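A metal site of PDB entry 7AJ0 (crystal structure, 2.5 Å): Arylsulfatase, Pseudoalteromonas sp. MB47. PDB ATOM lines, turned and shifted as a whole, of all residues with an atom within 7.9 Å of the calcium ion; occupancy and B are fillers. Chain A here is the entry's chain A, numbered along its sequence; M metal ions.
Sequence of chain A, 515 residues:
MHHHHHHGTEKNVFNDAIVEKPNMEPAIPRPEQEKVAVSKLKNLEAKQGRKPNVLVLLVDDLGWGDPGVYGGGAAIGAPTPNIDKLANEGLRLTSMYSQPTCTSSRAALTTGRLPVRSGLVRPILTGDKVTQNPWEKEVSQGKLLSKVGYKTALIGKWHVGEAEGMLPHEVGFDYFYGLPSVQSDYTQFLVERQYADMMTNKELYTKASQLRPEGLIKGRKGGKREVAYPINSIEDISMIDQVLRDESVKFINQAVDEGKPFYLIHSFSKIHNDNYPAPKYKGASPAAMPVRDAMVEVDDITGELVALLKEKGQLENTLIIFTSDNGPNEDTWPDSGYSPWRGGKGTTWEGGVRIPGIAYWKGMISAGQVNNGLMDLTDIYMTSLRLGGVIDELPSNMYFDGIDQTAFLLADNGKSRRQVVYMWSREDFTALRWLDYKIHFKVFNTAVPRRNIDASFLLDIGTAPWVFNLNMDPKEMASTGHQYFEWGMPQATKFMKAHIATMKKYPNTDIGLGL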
ATOM      1  N   LEU A  58     -10.263 -14.568 -26.398  1.00  0.00           N
ATOM      2  CA  LEU A  58     -10.070 -15.781 -25.598  1.00  0.00           C
ATOM      3  C   LEU A  58      -9.347 -16.799 -26.466  1.00  0.00           C
ATOM      4  O   LEU A  58      -9.943 -17.406 -27.357  1.00  0.00           O
ATOM      5  CB  LEU A  58     -11.408 -16.312 -25.107  1.00  0.00           C
ATOM      6  CG  LEU A  58     -11.381 -17.407 -24.050  1.00  0.00           C
ATOM      7  CD1 LEU A  58     -10.736 -16.931 -22.756  1.00  0.00           C
ATOM      8  CD2 LEU A  58     -12.805 -17.884 -23.794  1.00  0.00           C
ATOM      9  N   VAL A  59      -8.061 -16.990 -26.198  1.00  0.00           N
ATOM     10  CA  VAL A  59      -7.263 -17.989 -26.892  1.00  0.00           C
ATOM     11  C   VAL A  59      -7.373 -19.307 -26.134  1.00  0.00           C
ATOM     12  O   VAL A  59      -7.459 -19.330 -24.894  1.00  0.00           O
ATOM     13  CB  VAL A  59      -5.793 -17.545 -27.023  1.00  0.00           C
ATOM     14  CG1 VAL A  59      -5.023 -18.504 -27.913  1.00  0.00           C
ATOM     15  CG2 VAL A  59      -5.724 -16.128 -27.571  1.00  0.00           C
ATOM     16  N   ASP A  60      -7.378 -20.409 -26.873  1.00  0.00           N
ATOM     17  CA  ASP A  60      -7.586 -21.732 -26.302  1.00  0.00           C
ATOM     18  C   ASP A  60      -6.245 -22.378 -25.972  1.00  0.00           C
ATOM     19  O   ASP A  60      -5.360 -22.453 -26.822  1.00  0.00           O
ATOM     20  CB  ASP A  60      -8.380 -22.612 -27.275  1.00  0.00           C
ATOM     21  CG  ASP A  60      -8.989 -23.835 -26.613  1.00  0.00           C
ATOM     22  OD1 ASP A  60      -8.803 -24.016 -25.394  1.00  0.00           O
ATOM     23  OD2 ASP A  60      -9.659 -24.610 -27.312  1.00  0.00           O
ATOM     24  N   ASP A  61      -6.101 -22.840 -24.719  1.00  0.00           N
ATOM     25  CA  ASP A  61      -4.945 -23.614 -24.291  1.00  0.00           C
ATOM     26  C   ASP A  61      -3.644 -22.847 -24.497  1.00  0.00           C
ATOM     27  O   ASP A  61      -2.614 -23.414 -24.872  1.00  0.00           O
ATOM     28  CB  ASP A  61      -4.883 -24.961 -25.010  1.00  0.00           C
ATOM     29  CG  ASP A  61      -6.012 -25.886 -24.609  1.00  0.00           C
ATOM     30  OD1 ASP A  61      -6.839 -25.488 -23.768  1.00  0.00           O
ATOM     31  OD2 ASP A  61      -6.075 -27.025 -25.125  1.00  0.00           O
ATOM     32  N   LEU A  62      -3.671 -21.542 -24.228  1.00  0.00           N
ATOM     33  CA  LEU A  62      -2.501 -20.685 -24.369  1.00  0.00           C
ATOM     34  C   LEU A  62      -1.774 -20.605 -23.030  1.00  0.00           C
ATOM     35  O   LEU A  62      -2.391 -20.289 -21.999  1.00  0.00           O
ATOM     36  CB  LEU A  62      -2.905 -19.297 -24.837  1.00  0.00           C
ATOM     37  CG  LEU A  62      -1.761 -18.330 -25.160  1.00  0.00           C
ATOM     38  CD1 LEU A  62      -1.108 -18.710 -26.478  1.00  0.00           C
ATOM     39  CD2 LEU A  62      -2.239 -16.887 -25.165  1.00  0.00           C
ATOM     40  N   GLN A  99      -9.708 -21.746 -14.805  1.00  0.00           N
ATOM     41  CA  GLN A  99      -9.928 -23.113 -14.346  1.00  0.00           C
ATOM     42  C   GLN A  99      -8.964 -24.038 -15.079  1.00  0.00           C
ATOM     43  O   GLN A  99      -8.331 -23.667 -16.060  1.00  0.00           O
ATOM     44  CB  GLN A  99     -11.377 -23.515 -14.586  1.00  0.00           C
ATOM     45  CG  GLN A  99     -12.376 -22.534 -13.979  1.00  0.00           C
ATOM     46  CD  GLN A  99     -12.197 -22.390 -12.473  1.00  0.00           C
ATOM     47  OE1 GLN A  99     -12.321 -23.357 -11.722  1.00  0.00           O
ATOM     48  NE2 GLN A  99     -11.894 -21.175 -12.033  1.00  0.00           N
ATOM     49  N   PRO A 100      -8.828 -25.292 -14.624  1.00  0.00           N
ATOM     50  CA  PRO A 100      -7.829 -26.184 -15.223  1.00  0.00           C
ATOM     51  C   PRO A 100      -8.210 -26.770 -16.579  1.00  0.00           C
ATOM     52  O   PRO A 100      -7.326 -27.328 -17.235  1.00  0.00           O
ATOM     53  CB  PRO A 100      -7.670 -27.303 -14.170  1.00  0.00           C
ATOM     54  CG  PRO A 100      -8.277 -26.763 -12.924  1.00  0.00           C
ATOM     55  CD  PRO A 100      -9.377 -25.854 -13.374  1.00  0.00           C
ATOM     56  N   THR A 101      -9.467 -26.663 -17.016  1.00  0.00           N
ATOM     57  CA  THR A 101      -9.887 -27.295 -18.258  1.00  0.00           C
ATOM     58  C   THR A 101     -10.871 -26.392 -19.000  1.00  0.00           C
ATOM     59  O   THR A 101     -11.382 -25.415 -18.452  1.00  0.00           O
ATOM     60  CB  THR A 101     -10.512 -28.675 -18.000  1.00  0.00           C
ATOM     61  OG1 THR A 101     -11.518 -28.569 -16.986  1.00  0.00           O
ATOM     62  CG2 THR A 101      -9.452 -29.665 -17.554  1.00  0.00           C
ATOM     63  N   CYS A 102     -11.143 -26.759 -20.257  1.00  0.00           N
ATOM     64  CA  CYS A 102     -11.827 -25.870 -21.183  1.00  0.00           C
ATOM     65  C   CYS A 102     -13.233 -25.528 -20.700  1.00  0.00           C
ATOM     66  O   CYS A 102     -13.563 -24.363 -20.481  1.00  0.00           O
ATOM     67  CB  CYS A 102     -11.900 -26.501 -22.579  1.00  0.00           C
ATOM     68  SG  CYS A 102     -10.309 -26.916 -23.319  1.00  0.00           S
ATOM     69  N   THR A 103     -14.087 -26.545 -20.567  1.00  0.00           N
ATOM     70  CA  THR A 103     -15.490 -26.303 -20.231  1.00  0.00           C
ATOM     71  C   THR A 103     -15.627 -25.559 -18.917  1.00  0.00           C
ATOM     72  O   THR A 103     -16.499 -24.701 -18.766  1.00  0.00           O
ATOM     73  CB  THR A 103     -16.246 -27.632 -20.177  1.00  0.00           C
ATOM     74  OG1 THR A 103     -16.184 -28.280 -21.451  1.00  0.00           O
ATOM     75  CG2 THR A 103     -17.702 -27.398 -19.796  1.00  0.00           C
ATOM     76  N   SER A 105     -13.468 -23.429 -17.438  1.00  0.00           N
ATOM     77  CA  SER A 105     -13.068 -22.028 -17.540  1.00  0.00           C
ATOM     78  C   SER A 105     -14.073 -21.214 -18.341  1.00  0.00           C
ATOM     79  O   SER A 105     -14.324 -20.036 -18.022  1.00  0.00           O
ATOM     80  CB  SER A 105     -11.688 -21.933 -18.193  1.00  0.00           C
ATOM     81  OG  SER A 105     -10.677 -22.355 -17.297  1.00  0.00           O
ATOM     82  N   ARG A 106     -14.649 -21.803 -19.385  1.00  0.00           N
ATOM     83  CA  ARG A 106     -15.589 -21.050 -20.218  1.00  0.00           C
ATOM     84  C   ARG A 106     -16.933 -20.871 -19.529  1.00  0.00           C
ATOM     85  O   ARG A 106     -17.589 -19.840 -19.730  1.00  0.00           O
ATOM     86  CB  ARG A 106     -15.744 -21.765 -21.565  1.00  0.00           C
ATOM     87  CG  ARG A 106     -14.507 -21.581 -22.434  1.00  0.00           C
ATOM     88  CD  ARG A 106     -14.265 -22.740 -23.372  1.00  0.00           C
ATOM     89  NE  ARG A 106     -12.906 -22.662 -23.926  1.00  0.00           N
ATOM     90  CZ  ARG A 106     -12.543 -21.793 -24.869  1.00  0.00           C
ATOM     91  NH1 ARG A 106     -13.431 -20.953 -25.376  1.00  0.00           N
ATOM     92  NH2 ARG A 106     -11.294 -21.786 -25.308  1.00  0.00           N
ATOM     93  N   LYS A 157     -15.169 -20.885 -30.301  1.00  0.00           N
ATOM     94  CA  LYS A 157     -15.362 -22.113 -29.542  1.00  0.00           C
ATOM     95  C   LYS A 157     -16.318 -21.890 -28.376  1.00  0.00           C
ATOM     96  O   LYS A 157     -16.204 -20.891 -27.649  1.00  0.00           O
ATOM     97  CB  LYS A 157     -14.020 -22.630 -29.044  1.00  0.00           C
ATOM     98  CG  LYS A 157     -14.114 -23.861 -28.149  1.00  0.00           C
ATOM     99  CD  LYS A 157     -12.760 -24.192 -27.532  1.00  0.00           C
ATOM    100  CE  LYS A 157     -12.911 -25.183 -26.394  1.00  0.00           C
ATOM    101  NZ  LYS A 157     -11.644 -25.394 -25.643  1.00  0.00           N
ATOM    102  N   HIS A 159     -18.056 -25.076 -26.240  1.00  0.00           N
ATOM    103  CA  HIS A 159     -17.598 -26.167 -25.376  1.00  0.00           C
ATOM    104  C   HIS A 159     -18.171 -26.046 -23.968  1.00  0.00           C
ATOM    105  O   HIS A 159     -17.551 -26.490 -22.990  1.00  0.00           O
ATOM    106  CB  HIS A 159     -16.069 -26.194 -25.318  1.00  0.00           C
ATOM    107  CG  HIS A 159     -15.489 -27.567 -25.152  1.00  0.00           C
ATOM    108  ND1 HIS A 159     -14.169 -27.782 -24.815  1.00  0.00           N
ATOM    109  CD2 HIS A 159     -16.056 -28.788 -25.276  1.00  0.00           C
ATOM    110  CE1 HIS A 159     -13.952 -29.085 -24.728  1.00  0.00           C
ATOM    111  NE2 HIS A 159     -15.073 -29.716 -25.016  1.00  0.00           N
ATOM    112  N   VAL A 182     -15.350 -28.562 -29.879  1.00  0.00           N
ATOM    113  CA  VAL A 182     -13.932 -28.216 -29.753  1.00  0.00           C
ATOM    114  C   VAL A 182     -13.199 -28.718 -30.983  1.00  0.00           C
ATOM    115  O   VAL A 182     -13.665 -29.604 -31.677  1.00  0.00           O
ATOM    116  CB  VAL A 182     -13.349 -28.814 -28.443  1.00  0.00           C
ATOM    117  CG1 VAL A 182     -13.490 -30.336 -28.429  1.00  0.00           C
ATOM    118  CG2 VAL A 182     -11.905 -28.404 -28.238  1.00  0.00           C
ATOM    119  N   PHE A 268     -11.095 -17.927 -30.057  1.00  0.00           N
ATOM    120  CA  PHE A 268     -10.283 -18.640 -31.042  1.00  0.00           C
ATOM    121  C   PHE A 268     -10.444 -20.153 -30.864  1.00  0.00           C
ATOM    122  O   PHE A 268     -10.572 -20.658 -29.751  1.00  0.00           O
ATOM    123  CB  PHE A 268      -8.801 -18.292 -30.897  1.00  0.00           C
ATOM    124  CG  PHE A 268      -8.459 -16.865 -31.195  1.00  0.00           C
ATOM    125  CD1 PHE A 268      -8.162 -16.480 -32.490  1.00  0.00           C
ATOM    126  CD2 PHE A 268      -8.413 -15.925 -30.191  1.00  0.00           C
ATOM    127  CE1 PHE A 268      -7.837 -15.166 -32.773  1.00  0.00           C
ATOM    128  CE2 PHE A 268      -8.096 -14.608 -30.463  1.00  0.00           C
ATOM    129  CZ  PHE A 268      -7.800 -14.236 -31.763  1.00  0.00           C
ATOM    130  N   SER A 269     -10.412 -20.872 -31.983  1.00  0.00           N
ATOM    131  CA  SER A 269     -10.237 -22.313 -31.909  1.00  0.00           C
ATOM    132  C   SER A 269      -8.791 -22.661 -31.553  1.00  0.00           C
ATOM    133  O   SER A 269      -8.548 -23.620 -30.800  1.00  0.00           O
ATOM    134  CB  SER A 269     -10.622 -22.973 -33.234  1.00  0.00           C
ATOM    135  OG  SER A 269     -10.313 -24.366 -33.205  1.00  0.00           O
ATOM    136  N   LYS A 270      -7.837 -21.917 -32.078  1.00  0.00           N
ATOM    137  CA  LYS A 270      -6.442 -22.117 -31.718  1.00  0.00           C
ATOM    138  C   LYS A 270      -6.215 -21.722 -30.268  1.00  0.00           C
ATOM    139  O   LYS A 270      -6.917 -20.878 -29.717  1.00  0.00           O
ATOM    140  CB  LYS A 270      -5.537 -21.296 -32.647  1.00  0.00           C
ATOM    141  CG  LYS A 270      -5.492 -21.827 -34.062  1.00  0.00           C
ATOM    142  CD  LYS A 270      -5.110 -20.738 -35.054  1.00  0.00           C
ATOM    143  CE  LYS A 270      -5.025 -21.301 -36.475  1.00  0.00           C
ATOM    144  NZ  LYS A 270      -6.307 -21.936 -36.905  1.00  0.00           N
ATOM    145  N   ILE A 271      -5.219 -22.347 -29.616  1.00  0.00           N
ATOM    146  CA  ILE A 271      -4.302 -23.301 -30.219  1.00  0.00           C
ATOM    147  C   ILE A 271      -4.593 -24.730 -29.765  1.00  0.00           C
ATOM    148  O   ILE A 271      -3.675 -25.498 -29.469  1.00  0.00           O
ATOM    149  CB  ILE A 271      -2.831 -22.931 -29.872  1.00  0.00           C
ATOM    150  CG1 ILE A 271      -2.629 -22.878 -28.356  1.00  0.00           C
ATOM    151  CG2 ILE A 271      -2.441 -21.605 -30.500  1.00  0.00           C
ATOM    152  CD1 ILE A 271      -1.183 -22.739 -27.934  1.00  0.00           C
ATOM    153  N   HIS A 272      -5.872 -25.076 -29.699  1.00  0.00           N
ATOM    154  CA  HIS A 272      -6.257 -26.439 -29.363  1.00  0.00           C
ATOM    155  C   HIS A 272      -5.802 -27.394 -30.457  1.00  0.00           C
ATOM    156  O   HIS A 272      -5.789 -27.056 -31.646  1.00  0.00           O
ATOM    157  CB  HIS A 272      -7.769 -26.532 -29.179  1.00  0.00           C
ATOM    158  CG  HIS A 272      -8.198 -27.635 -28.271  1.00  0.00           C
ATOM    159  ND1 HIS A 272      -8.101 -28.968 -28.598  1.00  0.00           N
ATOM    160  CD2 HIS A 272      -8.753 -27.599 -27.031  1.00  0.00           C
ATOM    161  CE1 HIS A 272      -8.566 -29.706 -27.600  1.00  0.00           C
ATOM    162  NE2 HIS A 272      -8.966 -28.897 -26.644  1.00  0.00           N
ATOM    163  N   SER A 324      -6.553 -16.370 -21.811  1.00  0.00           N
ATOM    164  CA  SER A 324      -6.665 -17.774 -22.168  1.00  0.00           C
ATOM    165  C   SER A 324      -7.696 -18.440 -21.255  1.00  0.00           C
ATOM    166  O   SER A 324      -8.116 -17.882 -20.249  1.00  0.00           O
ATOM    167  CB  SER A 324      -5.313 -18.478 -22.046  1.00  0.00           C
ATOM    168  OG  SER A 324      -5.436 -19.878 -22.249  1.00  0.00           O
ATOM    169  N   ASP A 325      -8.098 -19.659 -21.630  1.00  0.00           N
ATOM    170  CA  ASP A 325      -9.045 -20.408 -20.809  1.00  0.00           C
ATOM    171  C   ASP A 325      -8.377 -21.437 -19.911  1.00  0.00           C
ATOM    172  O   ASP A 325      -8.988 -21.858 -18.925  1.00  0.00           O
ATOM    173  CB  ASP A 325     -10.080 -21.103 -21.700  1.00  0.00           C
ATOM    174  CG  ASP A 325      -9.537 -22.331 -22.406  1.00  0.00           C
ATOM    175  OD1 ASP A 325      -8.327 -22.361 -22.735  1.00  0.00           O
ATOM    176  OD2 ASP A 325     -10.328 -23.264 -22.624  1.00  0.00           O
ATOM    177  N   ASN A 326      -7.147 -21.826 -20.199  1.00  0.00           N
ATOM    178  CA  ASN A 326      -6.390 -22.702 -19.314  1.00  0.00           C
ATOM    179  C   ASN A 326      -4.951 -22.763 -19.827  1.00  0.00           C
ATOM    180  O   ASN A 326      -4.611 -22.161 -20.845  1.00  0.00           O
ATOM    181  CB  ASN A 326      -7.015 -24.091 -19.217  1.00  0.00           C
ATOM    182  CG  ASN A 326      -7.315 -24.691 -20.571  1.00  0.00           C
ATOM    183  OD1 ASN A 326      -8.472 -24.790 -20.977  1.00  0.00           O
ATOM    184  ND2 ASN A 326      -6.269 -25.098 -21.287  1.00  0.00           N
ATOM    185  N   GLY A 327      -4.113 -23.501 -19.101  1.00  0.00           N
ATOM    186  CA  GLY A 327      -2.711 -23.604 -19.437  1.00  0.00           C
ATOM    187  C   GLY A 327      -2.475 -24.523 -20.613  1.00  0.00           C
ATOM    188  O   GLY A 327      -3.393 -25.097 -21.214  1.00  0.00           O
ATOM    189  N   ASN A 329      -1.704 -27.497 -23.135  1.00  0.00           N
ATOM    190  CA  ASN A 329      -2.027 -28.919 -23.214  1.00  0.00           C
ATOM    191  C   ASN A 329      -0.748 -29.674 -23.572  1.00  0.00           C
ATOM    192  O   ASN A 329      -0.472 -29.961 -24.735  1.00  0.00           O
ATOM    193  CB  ASN A 329      -3.121 -29.166 -24.241  1.00  0.00           C
ATOM    194  CG  ASN A 329      -3.595 -30.609 -24.261  1.00  0.00           C
ATOM    195  OD1 ASN A 329      -2.965 -31.477 -23.661  1.00  0.00           O
ATOM    196  ND2 ASN A 329      -4.704 -30.864 -24.942  1.00  0.00           N
ATOM    197  N   LYS A 345      -2.428 -27.895 -18.416  1.00  0.00           N
ATOM    198  CA  LYS A 345      -3.866 -28.146 -18.488  1.00  0.00           C
ATOM    199  C   LYS A 345      -4.216 -29.460 -17.807  1.00  0.00           C
ATOM    200  O   LYS A 345      -3.502 -30.462 -17.936  1.00  0.00           O
ATOM    201  CB  LYS A 345      -4.313 -28.178 -19.955  1.00  0.00           C
ATOM    202  CG  LYS A 345      -5.801 -28.317 -20.173  1.00  0.00           C
ATOM    203  CD  LYS A 345      -6.075 -28.553 -21.645  1.00  0.00           C
ATOM    204  CE  LYS A 345      -7.554 -28.485 -21.969  1.00  0.00           C
ATOM    205  NZ  LYS A 345      -7.794 -28.722 -23.426  1.00  0.00           N
HETATM  206 CA    CA M   1      -8.953 -24.756 -23.351  1.00  0.00          CA
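The side-chain carboxylate of Asp 325 sits close to the side-chain amino group of Lys 157, 3.9 Å away. The side-chain carboxylate (OD2) of Asp 325 lies close to the guanidinium group (NE) of Arg 106, 3.0 Å away. N of Asp 325 lies within hydrogen-bond range of O of Val 59, at 3.3 Å. The side-chain carboxylate (OD2) of Asp 60 is in salt-bridge range of the side-chain amino group (NZ) of Lys 157 (2.7 Å). The side-chain carboxylate (OD2) of Asp 60 is in salt-bridge range of the guanidinium group (NH2) of Arg 106, at 3.8 Å. O of Asp 60 sits at hydrogen-bond distance from N of Ile 271, 2.8 Å away. The side-chain carboxylate (OD2) of Asp 61 lies within salt-bridge range of the side-chain amino group (NZ) of Lys 345 (3.0 Å). The side-chain sulfur (SG) of Cys 102 lies close to the side-chain amino group (NZ) of Lys 345, at 3.1 Å.
Merely in contact with the calcium ion: Lys 157.
The calcium ion is bound by OD2 of Asp 325 (2.2 Å), OD1 of Asp 60 (2.2 Å), OD1 of Asp 61 (2.3 Å), OD1 of Asn 326 (2.4 Å), OD1 of Asp 325 (2.6 Å) and SG of Cys 102 (2.6 Å).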
